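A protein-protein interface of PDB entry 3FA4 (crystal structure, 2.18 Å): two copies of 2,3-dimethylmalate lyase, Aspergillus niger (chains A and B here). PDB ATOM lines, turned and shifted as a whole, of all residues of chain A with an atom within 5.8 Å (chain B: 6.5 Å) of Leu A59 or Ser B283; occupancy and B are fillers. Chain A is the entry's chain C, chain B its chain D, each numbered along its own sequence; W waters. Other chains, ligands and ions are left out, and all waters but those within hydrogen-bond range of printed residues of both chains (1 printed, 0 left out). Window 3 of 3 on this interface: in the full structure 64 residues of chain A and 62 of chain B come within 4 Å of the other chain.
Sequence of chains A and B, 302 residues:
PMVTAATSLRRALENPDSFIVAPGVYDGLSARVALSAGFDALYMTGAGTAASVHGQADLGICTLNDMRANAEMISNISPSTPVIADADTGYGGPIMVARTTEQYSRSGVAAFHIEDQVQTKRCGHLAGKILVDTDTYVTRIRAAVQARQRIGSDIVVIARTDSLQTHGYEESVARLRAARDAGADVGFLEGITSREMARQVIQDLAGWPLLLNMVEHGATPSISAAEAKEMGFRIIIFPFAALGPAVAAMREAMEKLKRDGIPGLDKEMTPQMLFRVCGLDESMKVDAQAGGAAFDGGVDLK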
ATOM      1  N   ALA A  50     -20.044 -24.490  22.477  1.00  0.00           N
ATOM      2  CA  ALA A  50     -20.524 -23.230  21.903  1.00  0.00           C
ATOM      3  C   ALA A  50     -21.193 -23.317  20.553  1.00  0.00           C
ATOM      4  O   ALA A  50     -22.249 -22.695  20.317  1.00  0.00           O
ATOM      5  CB  ALA A  50     -19.361 -22.249  21.814  1.00  0.00           C
ATOM      6  N   GLN A  56     -22.613 -20.734  17.669  1.00  0.00           N
ATOM      7  CA  GLN A  56     -21.843 -19.500  17.831  1.00  0.00           C
ATOM      8  C   GLN A  56     -20.313 -19.806  17.932  1.00  0.00           C
ATOM      9  O   GLN A  56     -19.955 -20.906  18.303  1.00  0.00           O
ATOM     10  CB  GLN A  56     -22.326 -18.875  19.132  1.00  0.00           C
ATOM     11  CG  GLN A  56     -22.315 -17.479  19.127  1.00  0.00           C
ATOM     12  CD  GLN A  56     -23.492 -16.928  18.394  1.00  0.00           C
ATOM     13  OE1 GLN A  56     -24.530 -17.599  18.241  1.00  0.00           O
ATOM     14  NE2 GLN A  56     -23.347 -15.709  17.909  1.00  0.00           N
ATOM     15  N   ALA A  57     -19.416 -18.861  17.571  1.00  0.00           N
ATOM     16  CA  ALA A  57     -17.963 -19.085  17.751  1.00  0.00           C
ATOM     17  C   ALA A  57     -17.557 -19.058  19.225  1.00  0.00           C
ATOM     18  O   ALA A  57     -18.316 -18.584  20.070  1.00  0.00           O
ATOM     19  CB  ALA A  57     -17.120 -18.101  16.903  1.00  0.00           C
ATOM     20  N   ASP A  58     -16.356 -19.570  19.531  1.00  0.00           N
ATOM     21  CA  ASP A  58     -15.863 -19.702  20.904  1.00  0.00           C
ATOM     22  C   ASP A  58     -15.531 -18.322  21.534  1.00  0.00           C
ATOM     23  O   ASP A  58     -14.369 -17.861  21.546  1.00  0.00           O
ATOM     24  CB  ASP A  58     -14.680 -20.635  20.934  1.00  0.00           C
ATOM     25  CG  ASP A  58     -14.405 -21.186  22.338  1.00  0.00           C
ATOM     26  OD1 ASP A  58     -13.264 -21.650  22.599  1.00  0.00           O
ATOM     27  OD2 ASP A  58     -15.336 -21.181  23.172  1.00  0.00           O
ATOM     28  N   LEU A  59     -16.571 -17.636  22.012  1.00  0.00           N
ATOM     29  CA  LEU A  59     -16.439 -16.272  22.371  1.00  0.00           C
ATOM     30  C   LEU A  59     -16.796 -16.017  23.817  1.00  0.00           C
ATOM     31  O   LEU A  59     -17.063 -14.856  24.150  1.00  0.00           O
ATOM     32  CB  LEU A  59     -17.341 -15.431  21.420  1.00  0.00           C
ATOM     33  CG  LEU A  59     -16.913 -15.324  19.923  1.00  0.00           C
ATOM     34  CD1 LEU A  59     -17.950 -14.704  18.996  1.00  0.00           C
ATOM     35  CD2 LEU A  59     -15.524 -14.610  19.746  1.00  0.00           C
ATOM     36  N   GLY A  60     -16.794 -17.043  24.705  1.00  0.00           N
ATOM     37  CA  GLY A  60     -17.251 -16.839  26.127  1.00  0.00           C
ATOM     38  C   GLY A  60     -18.775 -16.588  26.246  1.00  0.00           C
ATOM     39  O   GLY A  60     -19.222 -15.869  27.141  1.00  0.00           O
ATOM     40  N   ILE A  61     -19.566 -17.201  25.351  1.00  0.00           N
ATOM     41  CA  ILE A  61     -21.031 -17.056  25.259  1.00  0.00           C
ATOM     42  C   ILE A  61     -21.751 -18.163  26.009  1.00  0.00           C
ATOM     43  O   ILE A  61     -22.971 -18.126  26.185  1.00  0.00           O
ATOM     44  CB  ILE A  61     -21.469 -17.251  23.806  1.00  0.00           C
ATOM     45  CG1 ILE A  61     -20.847 -16.173  22.930  1.00  0.00           C
ATOM     46  CG2 ILE A  61     -22.994 -17.401  23.704  1.00  0.00           C
ATOM     47  CD1 ILE A  61     -21.351 -14.807  23.182  1.00  0.00           C
ATOM     48  N   ARG B  32     -26.121 -24.032  11.004  1.00  0.00           N
ATOM     49  CA  ARG B  32     -25.264 -23.049  10.343  1.00  0.00           C
ATOM     50  C   ARG B  32     -24.942 -23.557   8.944  1.00  0.00           C
ATOM     51  O   ARG B  32     -25.023 -22.828   7.965  1.00  0.00           O
ATOM     52  CB  ARG B  32     -23.935 -22.859  11.151  1.00  0.00           C
ATOM     53  CG  ARG B  32     -24.118 -21.996  12.453  1.00  0.00           C
ATOM     54  CD  ARG B  32     -24.474 -20.510  12.103  1.00  0.00           C
ATOM     55  NE  ARG B  32     -24.422 -19.695  13.324  1.00  0.00           N
ATOM     56  CZ  ARG B  32     -24.516 -18.377  13.373  1.00  0.00           C
ATOM     57  NH1 ARG B  32     -24.663 -17.673  12.251  1.00  0.00           N
ATOM     58  NH2 ARG B  32     -24.523 -17.758  14.557  1.00  0.00           N
ATOM     59  N   CYS B 278     -19.779 -20.639  12.086  1.00  0.00           N
ATOM     60  CA  CYS B 278     -20.696 -20.198  13.147  1.00  0.00           C
ATOM     61  C   CYS B 278     -20.726 -18.708  13.380  1.00  0.00           C
ATOM     62  O   CYS B 278     -20.806 -18.308  14.558  1.00  0.00           O
ATOM     63  CB  CYS B 278     -20.340 -20.807  14.524  1.00  0.00           C
ATOM     64  SG  CYS B 278     -20.407 -22.584  14.586  1.00  0.00           S
ATOM     65  N   GLY B 279     -20.579 -17.908  12.313  1.00  0.00           N
ATOM     66  CA  GLY B 279     -20.885 -16.490  12.342  1.00  0.00           C
ATOM     67  C   GLY B 279     -19.908 -15.511  12.981  1.00  0.00           C
ATOM     68  O   GLY B 279     -20.297 -14.375  13.314  1.00  0.00           O
ATOM     69  N   LEU B 280     -18.648 -15.914  13.139  1.00  0.00           N
ATOM     70  CA  LEU B 280     -17.618 -15.008  13.705  1.00  0.00           C
ATOM     71  C   LEU B 280     -17.660 -13.543  13.229  1.00  0.00           C
ATOM     72  O   LEU B 280     -17.581 -12.631  14.060  1.00  0.00           O
ATOM     73  CB  LEU B 280     -16.197 -15.546  13.498  1.00  0.00           C
ATOM     74  CG  LEU B 280     -14.991 -14.758  14.040  1.00  0.00           C
ATOM     75  CD1 LEU B 280     -15.263 -14.512  15.538  1.00  0.00           C
ATOM     76  CD2 LEU B 280     -13.598 -15.487  13.822  1.00  0.00           C
ATOM     77  N   ASP B 281     -17.704 -13.317  11.916  1.00  0.00           N
ATOM     78  CA  ASP B 281     -17.646 -11.957  11.360  1.00  0.00           C
ATOM     79  C   ASP B 281     -18.789 -11.113  11.854  1.00  0.00           C
ATOM     80  O   ASP B 281     -18.570  -9.985  12.283  1.00  0.00           O
ATOM     81  CB  ASP B 281     -17.648 -11.969   9.818  1.00  0.00           C
ATOM     82  CG  ASP B 281     -16.393 -12.681   9.215  1.00  0.00           C
ATOM     83  OD1 ASP B 281     -15.497 -13.203   9.957  1.00  0.00           O
ATOM     84  OD2 ASP B 281     -16.307 -12.713   7.964  1.00  0.00           O
ATOM     85  N   GLU B 282     -19.996 -11.670  11.793  1.00  0.00           N
ATOM     86  CA  GLU B 282     -21.212 -11.017  12.307  1.00  0.00           C
ATOM     87  C   GLU B 282     -21.160 -10.735  13.827  1.00  0.00           C
ATOM     88  O   GLU B 282     -21.411  -9.627  14.220  1.00  0.00           O
ATOM     89  CB  GLU B 282     -22.471 -11.818  11.920  1.00  0.00           C
ATOM     90  CG  GLU B 282     -22.340 -12.607  10.565  1.00  0.00           C
ATOM     91  CD  GLU B 282     -22.238 -11.703   9.313  1.00  0.00           C
ATOM     92  OE1 GLU B 282     -21.324 -11.964   8.438  1.00  0.00           O
ATOM     93  OE2 GLU B 282     -23.075 -10.730   9.215  1.00  0.00           O
ATOM     94  N   SER B 283     -20.784 -11.710  14.664  1.00  0.00           N
ATOM     95  CA  SER B 283     -20.341 -11.423  16.055  1.00  0.00           C
ATOM     96  C   SER B 283     -19.320 -10.251  16.262  1.00  0.00           C
ATOM     97  O   SER B 283     -19.443  -9.455  17.206  1.00  0.00           O
ATOM     98  CB  SER B 283     -19.815 -12.670  16.730  1.00  0.00           C
ATOM     99  OG  SER B 283     -20.876 -13.389  17.286  1.00  0.00           O
ATOM    100  N   MET B 284     -18.320 -10.115  15.400  1.00  0.00           N
ATOM    101  CA  MET B 284     -17.397  -8.996  15.532  1.00  0.00           C
ATOM    102  C   MET B 284     -17.950  -7.609  15.131  1.00  0.00           C
ATOM    103  O   MET B 284     -17.592  -6.586  15.738  1.00  0.00           O
ATOM    104  CB  MET B 284     -16.141  -9.352  14.788  1.00  0.00           C
ATOM    105  CG  MET B 284     -15.240 -10.136  15.656  1.00  0.00           C
ATOM    106  SD  MET B 284     -14.101 -10.983  14.615  1.00  0.00           S
ATOM    107  CE  MET B 284     -13.090  -9.660  13.879  1.00  0.00           C
ATOM    108  N   LYS B 285     -18.827  -7.576  14.122  1.00  0.00           N
ATOM    109  CA  LYS B 285     -19.537  -6.364  13.715  1.00  0.00           C
ATOM    110  C   LYS B 285     -20.399  -5.835  14.852  1.00  0.00           C
ATOM    111  O   LYS B 285     -20.320  -4.649  15.192  1.00  0.00           O
ATOM    112  CB  LYS B 285     -20.413  -6.647  12.507  1.00  0.00           C
ATOM    113  CG  LYS B 285     -19.774  -6.284  11.175  1.00  0.00           C
ATOM    114  CD  LYS B 285     -20.451  -7.015  10.011  1.00  0.00           C
ATOM    115  CE  LYS B 285     -21.921  -7.211  10.297  1.00  0.00           C
ATOM    116  NZ  LYS B 285     -22.505  -8.520   9.735  1.00  0.00           N
ATOM    117  N   VAL B 286     -21.201  -6.727  15.432  1.00  0.00           N
ATOM    118  CA  VAL B 286     -22.042  -6.437  16.612  1.00  0.00           C
ATOM    119  C   VAL B 286     -21.210  -5.833  17.710  1.00  0.00           C
ATOM    120  O   VAL B 286     -21.649  -4.875  18.337  1.00  0.00           O
ATOM    121  CB  VAL B 286     -22.735  -7.711  17.201  1.00  0.00           C
ATOM    122  CG1 VAL B 286     -23.188  -7.493  18.647  1.00  0.00           C
ATOM    123  CG2 VAL B 286     -23.880  -8.182  16.316  1.00  0.00           C
ATOM    124  N   ASP B 287     -20.030  -6.407  17.955  1.00  0.00           N
ATOM    125  CA  ASP B 287     -19.110  -5.842  18.948  1.00  0.00           C
ATOM    126  C   ASP B 287     -18.582  -4.440  18.600  1.00  0.00           C
ATOM    127  O   ASP B 287     -18.590  -3.564  19.449  1.00  0.00           O
ATOM    128  CB  ASP B 287     -17.920  -6.770  19.255  1.00  0.00           C
ATOM    129  CG  ASP B 287     -17.035  -6.188  20.351  1.00  0.00           C
ATOM    130  OD1 ASP B 287     -16.023  -5.510  20.043  1.00  0.00           O
ATOM    131  OD2 ASP B 287     -17.409  -6.321  21.541  1.00  0.00           O
ATOM    132  N   ALA B 288     -18.090  -4.261  17.364  1.00  0.00           N
ATOM    133  CA  ALA B 288     -17.571  -2.976  16.879  1.00  0.00           C
ATOM    134  C   ALA B 288     -18.701  -1.938  16.850  1.00  0.00           C
ATOM    135  O   ALA B 288     -18.449  -0.838  17.148  1.00  0.00           O
ATOM    136  CB  ALA B 288     -16.925  -3.101  15.489  1.00  0.00           C
HETATM  137  O   HOH W   1     -20.316 -16.348  16.626  1.00  0.00           O
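O of Cys B278 lies within hydrogen-bond range of N of Ala A57 (3.4 Å). The side-chain amide nitrogen (NE2) of Gln A56 lies within hydrogen-bond range of the side-chain hydroxyl (OG) of Ser B283, 3.4 Å away.
N of Gln A56 is in hydrogen-bond range of O of Ala A50.
OE1 of Gln A56 touches NH2 of Arg B32, at 3.7 Å. Gln A56 touches Cys B278. Leu A59 touches Ser B283 (CD1 to CB, 3.6 Å).
Of chain A, only Gln A56 (3.4 Å) and Leu A59 (3.6 Å) come within 4 Å of Ser B283. Of the printed residues of chain A, Cys B278 touches Gln A56 (3.6 Å) and Ala A57 (3.4 Å). Of the printed residues of chain B, Ala A57 touches Cys B278 (3.4 Å). The nearest residue of chain B that does not touch Leu A59 is Leu B280 (4.2 Å). The nearest residue of chain A that does not touch Ser B283 is Ala A57 (5.7 Å).
Of the 12 printed residues of chain B, 3 touch a printed residue of chain A. Of the 7 printed residues of chain A, 3 touch a printed residue of chain B. Hydrophobic or aromatic side chains of chain A that line the printed part of chain B: Leu A59. Among the printed residues, no Asp or Glu carboxylate lies within 4 Å of a Lys or Arg side-chain nitrogen of the other chain.
No position is printed for both chains.
Water W1 lies within hydrogen-bond range of N of Ala A57 (2.8 Å), O of Cys B278 (2.9 Å), OG of Ser B283 (3.1 Å) and NE2 of Gln A56 (3.4 Å).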
